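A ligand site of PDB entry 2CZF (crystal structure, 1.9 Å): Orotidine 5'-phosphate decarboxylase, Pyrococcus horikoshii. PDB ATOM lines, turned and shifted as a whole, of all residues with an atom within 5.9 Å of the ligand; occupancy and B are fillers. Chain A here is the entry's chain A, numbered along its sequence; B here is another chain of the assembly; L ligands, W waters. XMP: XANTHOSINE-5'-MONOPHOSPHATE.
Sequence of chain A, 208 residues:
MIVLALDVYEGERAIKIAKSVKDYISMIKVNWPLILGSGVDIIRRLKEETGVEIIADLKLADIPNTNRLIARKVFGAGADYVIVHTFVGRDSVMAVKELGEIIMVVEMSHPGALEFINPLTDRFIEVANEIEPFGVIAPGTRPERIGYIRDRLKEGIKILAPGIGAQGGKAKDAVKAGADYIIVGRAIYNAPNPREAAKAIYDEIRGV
The side-chain amino group of Lys 29 is in salt-bridge range of the side-chain carboxylate of Asp 57, 2.9 Å away.
The side-chain carboxylate (OD1) of Asp 7 lies within hydrogen-bond range of the side-chain amide nitrogen (ND2) of Asn 31 (3.1 Å).
The backbone carbonyl oxygen of Val 184 is in hydrogen-bond range of the backbone NH of Ala 5 (2.8 Å).
NZ of Lys 59 lies within salt-bridge range of OD1 of Asp 57.
NZ of Lys 59 is in salt-bridge range of OD2 of Asp 62 of chain B, 3.0 Å away.
The side-chain amino group (NZ) of Lys 29 sits at hydrogen-bond distance from an oxygen (O3') of the ligand (2.8 Å).
The backbone NH of Ser 109 lies within hydrogen-bond range of an oxygen (O6) of the ligand (3.2 Å).
OG of Ser 109 sits at hydrogen-bond distance from O6 of the ligand (2.8 Å).
The backbone NH (N) of Arg 186 sits close to an oxygen (O3P) of the ligand (3.3 Å).
NE of Arg 186 lies within salt-bridge range of O1P of the ligand (3.6 Å).
An oxygen (O3') of the ligand lies close to the side-chain carboxylate (OD2) of Asp 7, at 3.2 Å.
The backbone NH (N) of Gly 185 sits at hydrogen-bond distance from an oxygen (O2P) of the ligand, at 3.2 Å.
Merely in contact with the ligand: Ala 5 (3.3 Å), Lys 59 (3.7 Å), Ile 137 (3.7 Å), Pro 162 (3.1 Å), Gly 163 (3.96 Å), Ile 183 (3.9 Å) and Ile 63 of chain B (3.2 Å).
Hydrophobic or aromatic side chains within 4 Å of the ligand: Ala 5, Ile 137, Pro 162, Ile 183 and Ile 63 of chain B.
Of the 25 residues printed, 12 come within 4 Å of the ligand.
Water W2 lies within hydrogen-bond range of O2P of the ligand and N of Ala 187.
Water W1 lies within hydrogen-bond range of N of Ile 164 (2.6 Å), O of Ile 183 (2.9 Å), N of Gly 163 (2.9 Å) and O2P of the ligand (3.1 Å).
Water W3 lies within hydrogen-bond range of the side-chain amide nitrogen of Asn 31, an oxygen (O2') of the ligand and the side-chain amino group of Lys 29.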
ATOM      1  N   ALA A   5      33.836  -9.447  -5.181  1.00  0.00           N
ATOM      2  CA  ALA A   5      32.426  -9.228  -5.477  1.00  0.00           C
ATOM      3  C   ALA A   5      32.409  -8.390  -6.752  1.00  0.00           C
ATOM      4  O   ALA A   5      32.505  -7.161  -6.704  1.00  0.00           O
ATOM      5  CB  ALA A   5      31.767  -8.469  -4.339  1.00  0.00           C
ATOM      6  N   ASP A   7      30.737  -6.675  -8.618  1.00  0.00           N
ATOM      7  CA  ASP A   7      29.536  -5.873  -8.769  1.00  0.00           C
ATOM      8  C   ASP A   7      29.749  -4.684  -9.679  1.00  0.00           C
ATOM      9  O   ASP A   7      29.444  -3.544  -9.320  1.00  0.00           O
ATOM     10  CB  ASP A   7      29.037  -5.384  -7.422  1.00  0.00           C
ATOM     11  CG  ASP A   7      28.770  -6.530  -6.483  1.00  0.00           C
ATOM     12  OD1 ASP A   7      28.503  -7.635  -6.987  1.00  0.00           O
ATOM     13  OD2 ASP A   7      28.816  -6.318  -5.248  1.00  0.00           O
ATOM     14  N   LYS A  29      32.695 -13.734  -6.962  1.00  0.00           N
ATOM     15  CA  LYS A  29      31.273 -13.831  -6.637  1.00  0.00           C
ATOM     16  C   LYS A  29      30.437 -12.982  -7.596  1.00  0.00           C
ATOM     17  O   LYS A  29      30.700 -11.792  -7.757  1.00  0.00           O
ATOM     18  CB  LYS A  29      30.990 -13.358  -5.200  1.00  0.00           C
ATOM     19  CG  LYS A  29      29.497 -13.401  -4.813  1.00  0.00           C
ATOM     20  CD  LYS A  29      29.235 -12.968  -3.375  1.00  0.00           C
ATOM     21  CE  LYS A  29      29.160 -11.458  -3.219  1.00  0.00           C
ATOM     22  NZ  LYS A  29      28.027 -10.917  -4.017  1.00  0.00           N
ATOM     23  N   ASN A  31      26.367 -11.836  -8.928  1.00  0.00           N
ATOM     24  CA  ASN A  31      25.000 -11.754  -8.440  1.00  0.00           C
ATOM     25  C   ASN A  31      23.969 -11.738  -9.576  1.00  0.00           C
ATOM     26  O   ASN A  31      24.317 -11.838 -10.761  1.00  0.00           O
ATOM     27  CB  ASN A  31      24.832 -10.506  -7.570  1.00  0.00           C
ATOM     28  CG  ASN A  31      25.253  -9.240  -8.299  1.00  0.00           C
ATOM     29  OD1 ASN A  31      25.301  -9.206  -9.540  1.00  0.00           O
ATOM     30  ND2 ASN A  31      25.552  -8.188  -7.539  1.00  0.00           N
ATOM     31  N   ASP A  57      25.988 -15.689  -6.201  1.00  0.00           N
ATOM     32  CA  ASP A  57      25.240 -15.144  -5.090  1.00  0.00           C
ATOM     33  C   ASP A  57      23.799 -14.980  -5.534  1.00  0.00           C
ATOM     34  O   ASP A  57      23.398 -13.916  -5.990  1.00  0.00           O
ATOM     35  CB  ASP A  57      25.812 -13.780  -4.691  1.00  0.00           C
ATOM     36  CG  ASP A  57      25.210 -13.251  -3.420  1.00  0.00           C
ATOM     37  OD1 ASP A  57      24.328 -13.928  -2.857  1.00  0.00           O
ATOM     38  OD2 ASP A  57      25.628 -12.149  -2.981  1.00  0.00           O
ATOM     39  N   LYS A  59      21.067 -16.339  -3.506  1.00  0.00           N
ATOM     40  CA  LYS A  59      20.180 -16.385  -2.337  1.00  0.00           C
ATOM     41  C   LYS A  59      18.868 -17.106  -2.698  1.00  0.00           C
ATOM     42  O   LYS A  59      17.769 -16.597  -2.485  1.00  0.00           O
ATOM     43  CB  LYS A  59      19.901 -14.975  -1.802  1.00  0.00           C
ATOM     44  CG  LYS A  59      21.156 -14.350  -1.202  1.00  0.00           C
ATOM     45  CD  LYS A  59      20.885 -13.072  -0.429  1.00  0.00           C
ATOM     46  CE  LYS A  59      22.201 -12.467   0.045  1.00  0.00           C
ATOM     47  NZ  LYS A  59      23.033 -12.056  -1.116  1.00  0.00           N
ATOM     48  N   VAL A 105      22.840 -18.844   3.931  1.00  0.00           N
ATOM     49  CA  VAL A 105      22.655 -17.543   4.574  1.00  0.00           C
ATOM     50  C   VAL A 105      22.033 -17.754   5.967  1.00  0.00           C
ATOM     51  O   VAL A 105      20.914 -18.228   6.072  1.00  0.00           O
ATOM     52  CB  VAL A 105      21.683 -16.671   3.751  1.00  0.00           C
ATOM     53  CG1 VAL A 105      21.327 -15.417   4.537  1.00  0.00           C
ATOM     54  CG2 VAL A 105      22.322 -16.333   2.427  1.00  0.00           C
ATOM     55  N   GLU A 107      22.552 -15.165   8.542  1.00  0.00           N
ATOM     56  CA  GLU A 107      22.428 -13.814   9.128  1.00  0.00           C
ATOM     57  C   GLU A 107      22.653 -12.754   8.058  1.00  0.00           C
ATOM     58  O   GLU A 107      23.421 -12.972   7.123  1.00  0.00           O
ATOM     59  CB  GLU A 107      23.458 -13.639  10.243  1.00  0.00           C
ATOM     60  CG  GLU A 107      23.487 -12.232  10.850  1.00  0.00           C
ATOM     61  CD  GLU A 107      24.393 -12.146  12.064  1.00  0.00           C
ATOM     62  OE1 GLU A 107      24.258 -13.006  12.956  1.00  0.00           O
ATOM     63  OE2 GLU A 107      25.231 -11.220  12.129  1.00  0.00           O
ATOM     64  N   MET A 108      22.004 -11.586   8.191  1.00  0.00           N
ATOM     65  CA  MET A 108      22.159 -10.526   7.192  1.00  0.00           C
ATOM     66  C   MET A 108      22.468  -9.168   7.850  1.00  0.00           C
ATOM     67  O   MET A 108      22.239  -8.986   9.041  1.00  0.00           O
ATOM     68  CB  MET A 108      20.911 -10.467   6.307  1.00  0.00           C
ATOM     69  CG  MET A 108      20.706 -11.758   5.502  1.00  0.00           C
ATOM     70  SD  MET A 108      19.418 -11.611   4.251  1.00  0.00           S
ATOM     71  CE  MET A 108      20.277 -10.621   2.994  1.00  0.00           C
ATOM     72  N   SER A 109      23.000  -8.219   7.076  1.00  0.00           N
ATOM     73  CA  SER A 109      23.388  -6.962   7.691  1.00  0.00           C
ATOM     74  C   SER A 109      22.561  -5.704   7.447  1.00  0.00           C
ATOM     75  O   SER A 109      22.913  -4.650   7.952  1.00  0.00           O
ATOM     76  CB  SER A 109      24.859  -6.658   7.342  1.00  0.00           C
ATOM     77  OG  SER A 109      24.973  -6.084   6.061  1.00  0.00           O
ATOM     78  N   HIS A 110      21.471  -5.801   6.696  1.00  0.00           N
ATOM     79  CA  HIS A 110      20.644  -4.629   6.447  1.00  0.00           C
ATOM     80  C   HIS A 110      19.626  -4.467   7.605  1.00  0.00           C
ATOM     81  O   HIS A 110      19.330  -5.415   8.331  1.00  0.00           O
ATOM     82  CB  HIS A 110      19.913  -4.753   5.110  1.00  0.00           C
ATOM     83  CG  HIS A 110      18.989  -5.930   5.033  1.00  0.00           C
ATOM     84  ND1 HIS A 110      19.419  -7.227   5.187  1.00  0.00           N
ATOM     85  CD2 HIS A 110      17.644  -6.008   4.850  1.00  0.00           C
ATOM     86  CE1 HIS A 110      18.390  -8.051   5.109  1.00  0.00           C
ATOM     87  NE2 HIS A 110      17.299  -7.334   4.901  1.00  0.00           N
ATOM     88  N   ILE A 137      27.554 -17.487   5.179  1.00  0.00           N
ATOM     89  CA  ILE A 137      27.925 -16.077   5.088  1.00  0.00           C
ATOM     90  C   ILE A 137      27.762 -15.462   6.464  1.00  0.00           C
ATOM     91  O   ILE A 137      26.835 -15.801   7.201  1.00  0.00           O
ATOM     92  CB  ILE A 137      26.989 -15.285   4.135  1.00  0.00           C
ATOM     93  CG1 ILE A 137      27.147 -15.783   2.691  1.00  0.00           C
ATOM     94  CG2 ILE A 137      27.304 -13.799   4.247  1.00  0.00           C
ATOM     95  CD1 ILE A 137      28.407 -15.283   2.004  1.00  0.00           C
ATOM     96  N   PRO A 139      28.080 -11.501   7.975  1.00  0.00           N
ATOM     97  CA  PRO A 139      28.451 -10.088   7.801  1.00  0.00           C
ATOM     98  C   PRO A 139      29.627  -9.780   8.709  1.00  0.00           C
ATOM     99  O   PRO A 139      29.558 -10.019   9.917  1.00  0.00           O
ATOM    100  CB  PRO A 139      27.182  -9.341   8.197  1.00  0.00           C
ATOM    101  CG  PRO A 139      26.519 -10.299   9.178  1.00  0.00           C
ATOM    102  CD  PRO A 139      26.707 -11.629   8.499  1.00  0.00           C
ATOM    103  N   PRO A 162      31.322 -10.648   3.979  1.00  0.00           N
ATOM    104  CA  PRO A 162      31.212  -9.450   3.151  1.00  0.00           C
ATOM    105  C   PRO A 162      31.150  -8.251   4.102  1.00  0.00           C
ATOM    106  O   PRO A 162      31.143  -8.420   5.329  1.00  0.00           O
ATOM    107  CB  PRO A 162      29.900  -9.669   2.415  1.00  0.00           C
ATOM    108  CG  PRO A 162      29.068 -10.361   3.452  1.00  0.00           C
ATOM    109  CD  PRO A 162      30.030 -11.354   4.056  1.00  0.00           C
ATOM    110  N   GLY A 163      31.106  -7.033   3.557  1.00  0.00           N
ATOM    111  CA  GLY A 163      31.042  -5.861   4.412  1.00  0.00           C
ATOM    112  C   GLY A 163      32.282  -5.643   5.265  1.00  0.00           C
ATOM    113  O   GLY A 163      32.205  -5.330   6.462  1.00  0.00           O
ATOM    114  N   ILE A 164      33.445  -5.819   4.651  1.00  0.00           N
ATOM    115  CA  ILE A 164      34.700  -5.605   5.349  1.00  0.00           C
ATOM    116  C   ILE A 164      35.006  -4.109   5.243  1.00  0.00           C
ATOM    117  O   ILE A 164      34.927  -3.527   4.156  1.00  0.00           O
ATOM    118  CB  ILE A 164      35.843  -6.418   4.716  1.00  0.00           C
ATOM    119  CG1 ILE A 164      35.505  -7.912   4.806  1.00  0.00           C
ATOM    120  CG2 ILE A 164      37.151  -6.127   5.413  1.00  0.00           C
ATOM    121  CD1 ILE A 164      35.213  -8.399   6.213  1.00  0.00           C
ATOM    122  N   ILE A 183      34.887 -11.197   1.620  1.00  0.00           N
ATOM    123  CA  ILE A 183      34.304 -10.817   0.343  1.00  0.00           C
ATOM    124  C   ILE A 183      34.448  -9.321   0.191  1.00  0.00           C
ATOM    125  O   ILE A 183      33.877  -8.559   0.962  1.00  0.00           O
ATOM    126  CB  ILE A 183      32.803 -11.206   0.287  1.00  0.00           C
ATOM    127  CG1 ILE A 183      32.662 -12.711   0.443  1.00  0.00           C
ATOM    128  CG2 ILE A 183      32.199 -10.789  -1.060  1.00  0.00           C
ATOM    129  CD1 ILE A 183      31.222 -13.188   0.495  1.00  0.00           C
ATOM    130  N   VAL A 184      35.222  -8.916  -0.809  1.00  0.00           N
ATOM    131  CA  VAL A 184      35.451  -7.483  -1.048  1.00  0.00           C
ATOM    132  C   VAL A 184      35.028  -7.088  -2.450  1.00  0.00           C
ATOM    133  O   VAL A 184      35.335  -7.790  -3.419  1.00  0.00           O
ATOM    134  CB  VAL A 184      36.929  -7.098  -0.873  1.00  0.00           C
ATOM    135  CG1 VAL A 184      37.107  -5.601  -1.137  1.00  0.00           C
ATOM    136  CG2 VAL A 184      37.397  -7.449   0.536  1.00  0.00           C
ATOM    137  N   GLY A 185      34.329  -5.956  -2.551  1.00  0.00           N
ATOM    138  CA  GLY A 185      33.889  -5.477  -3.851  1.00  0.00           C
ATOM    139  C   GLY A 185      34.453  -4.087  -4.155  1.00  0.00           C
ATOM    140  O   GLY A 185      35.517  -3.966  -4.771  1.00  0.00           O
ATOM    141  N   ARG A 186      33.735  -3.055  -3.716  1.00  0.00           N
ATOM    142  CA  ARG A 186      34.131  -1.660  -3.941  1.00  0.00           C
ATOM    143  C   ARG A 186      35.628  -1.397  -3.807  1.00  0.00           C
ATOM    144  O   ARG A 186      36.323  -1.119  -4.790  1.00  0.00           O
ATOM    145  CB  ARG A 186      33.401  -0.740  -2.965  1.00  0.00           C
ATOM    146  CG  ARG A 186      31.900  -0.880  -2.957  1.00  0.00           C
ATOM    147  CD  ARG A 186      31.206   0.397  -2.522  1.00  0.00           C
ATOM    148  NE  ARG A 186      30.896   0.461  -1.095  1.00  0.00           N
ATOM    149  CZ  ARG A 186      30.066   1.361  -0.559  1.00  0.00           C
ATOM    150  NH1 ARG A 186      29.477   2.263  -1.344  1.00  0.00           N
ATOM    151  NH2 ARG A 186      29.826   1.363   0.749  1.00  0.00           N
ATOM    152  N   ALA A 187      36.119  -1.473  -2.566  1.00  0.00           N
ATOM    153  CA  ALA A 187      37.513  -1.210  -2.250  1.00  0.00           C
ATOM    154  C   ALA A 187      38.507  -1.796  -3.248  1.00  0.00           C
ATOM    155  O   ALA A 187      39.681  -1.442  -3.212  1.00  0.00           O
ATOM    156  CB  ALA A 187      37.824  -1.704  -0.845  1.00  0.00           C
ATOM    157  N   TYR A 189      37.403  -3.181  -7.027  1.00  0.00           N
ATOM    158  CA  TYR A 189      37.019  -2.836  -8.393  1.00  0.00           C
ATOM    159  C   TYR A 189      36.828  -1.340  -8.675  1.00  0.00           C
ATOM    160  O   TYR A 189      36.710  -0.937  -9.823  1.00  0.00           O
ATOM    161  CB  TYR A 189      35.772  -3.635  -8.834  1.00  0.00           C
ATOM    162  CG  TYR A 189      34.469  -3.293  -8.125  1.00  0.00           C
ATOM    163  CD1 TYR A 189      33.898  -2.029  -8.221  1.00  0.00           C
ATOM    164  CD2 TYR A 189      33.797  -4.256  -7.370  1.00  0.00           C
ATOM    165  CE1 TYR A 189      32.694  -1.718  -7.593  1.00  0.00           C
ATOM    166  CE2 TYR A 189      32.587  -3.958  -6.740  1.00  0.00           C
ATOM    167  CZ  TYR A 189      32.042  -2.690  -6.848  1.00  0.00           C
ATOM    168  OH  TYR A 189      30.847  -2.385  -6.237  1.00  0.00           O
ATOM    169  N   ASP B  62      17.049 -10.339  -1.068  1.00  0.00           N
ATOM    170  CA  ASP B  62      18.375  -9.795  -0.826  1.00  0.00           C
ATOM    171  C   ASP B  62      18.270  -8.465  -0.071  1.00  0.00           C
ATOM    172  O   ASP B  62      17.180  -8.044   0.306  1.00  0.00           O
ATOM    173  CB  ASP B  62      19.113  -9.593  -2.158  1.00  0.00           C
ATOM    174  CG  ASP B  62      20.600  -9.917  -2.045  1.00  0.00           C
ATOM    175  OD1 ASP B  62      21.262  -9.399  -1.127  1.00  0.00           O
ATOM    176  OD2 ASP B  62      21.099 -10.698  -2.891  1.00  0.00           O
ATOM    177  N   ILE B  63      19.415  -7.810   0.148  1.00  0.00           N
ATOM    178  CA  ILE B  63      19.430  -6.510   0.833  1.00  0.00           C
ATOM    179  C   ILE B  63      18.744  -5.474  -0.059  1.00  0.00           C
ATOM    180  O   ILE B  63      18.636  -5.672  -1.272  1.00  0.00           O
ATOM    181  CB  ILE B  63      20.882  -6.070   1.151  1.00  0.00           C
ATOM    182  CG1 ILE B  63      21.666  -5.884  -0.153  1.00  0.00           C
ATOM    183  CG2 ILE B  63      21.564  -7.108   2.019  1.00  0.00           C
ATOM    184  CD1 ILE B  63      23.059  -5.295   0.060  1.00  0.00           C
ATOM    185  N   THR B  66      20.410  -4.380  -3.505  1.00  0.00           N
ATOM    186  CA  THR B  66      20.439  -5.442  -4.509  1.00  0.00           C
ATOM    187  C   THR B  66      19.041  -5.791  -5.008  1.00  0.00           C
ATOM    188  O   THR B  66      18.843  -6.056  -6.194  1.00  0.00           O
ATOM    189  CB  THR B  66      21.151  -6.679  -3.967  1.00  0.00           C
ATOM    190  OG1 THR B  66      22.503  -6.337  -3.651  1.00  0.00           O
ATOM    191  CG2 THR B  66      21.159  -7.792  -5.009  1.00  0.00           C
HETATM  192  P   XMP L   1      31.100  -3.841  -0.590  1.00  0.00           P
HETATM  193  O1P XMP L   1      30.639  -2.839   0.397  1.00  0.00           O
HETATM  194  O2P XMP L   1      32.676  -4.152  -0.448  1.00  0.00           O
HETATM  195  O5' XMP L   1      30.353  -5.249  -0.463  1.00  0.00           O
HETATM  196  O3P XMP L   1      30.885  -3.349  -2.110  1.00  0.00           O
HETATM  197  C5' XMP L   1      31.022  -6.443  -0.881  1.00  0.00           C
HETATM  198  C4' XMP L   1      30.036  -7.600  -1.056  1.00  0.00           C
HETATM  199  O4' XMP L   1      29.234  -7.687   0.135  1.00  0.00           O
HETATM  200  C1' XMP L   1      27.873  -7.804  -0.311  1.00  0.00           C
HETATM  201  N9  XMP L   1      26.939  -7.478   0.785  1.00  0.00           N
HETATM  202  C4  XMP L   1      26.202  -8.355   1.455  1.00  0.00           C
HETATM  203  N3  XMP L   1      26.075  -9.757   1.348  1.00  0.00           N
HETATM  204  N1  XMP L   1      24.462  -9.732   3.150  1.00  0.00           N
HETATM  205  C2  XMP L   1      25.203 -10.444   2.199  1.00  0.00           C
HETATM  206  O2  XMP L   1      25.101 -11.666   2.123  1.00  0.00           O
HETATM  207  C6  XMP L   1      24.597  -8.336   3.239  1.00  0.00           C
HETATM  208  O6  XMP L   1      23.927  -7.710   4.068  1.00  0.00           O
HETATM  209  C5  XMP L   1      25.468  -7.655   2.401  1.00  0.00           C
HETATM  210  N7  XMP L   1      25.788  -6.369   2.270  1.00  0.00           N
HETATM  211  C8  XMP L   1      26.683  -6.268   1.285  1.00  0.00           C
HETATM  212  C2' XMP L   1      27.829  -6.806  -1.469  1.00  0.00           C
HETATM  213  O2' XMP L   1      26.677  -7.063  -2.276  1.00  0.00           O
HETATM  214  C3' XMP L   1      29.073  -7.306  -2.209  1.00  0.00           C
HETATM  215  O3' XMP L   1      28.777  -8.511  -2.903  1.00  0.00           O
HETATM  216  O   HOH W   1      33.351  -5.908   2.026  1.00  0.00           O
HETATM  217  O   HOH W   2      35.054  -2.743   0.069  1.00  0.00           O
HETATM  218  O   HOH W   3      25.680  -8.789  -4.713  1.00  0.00           O
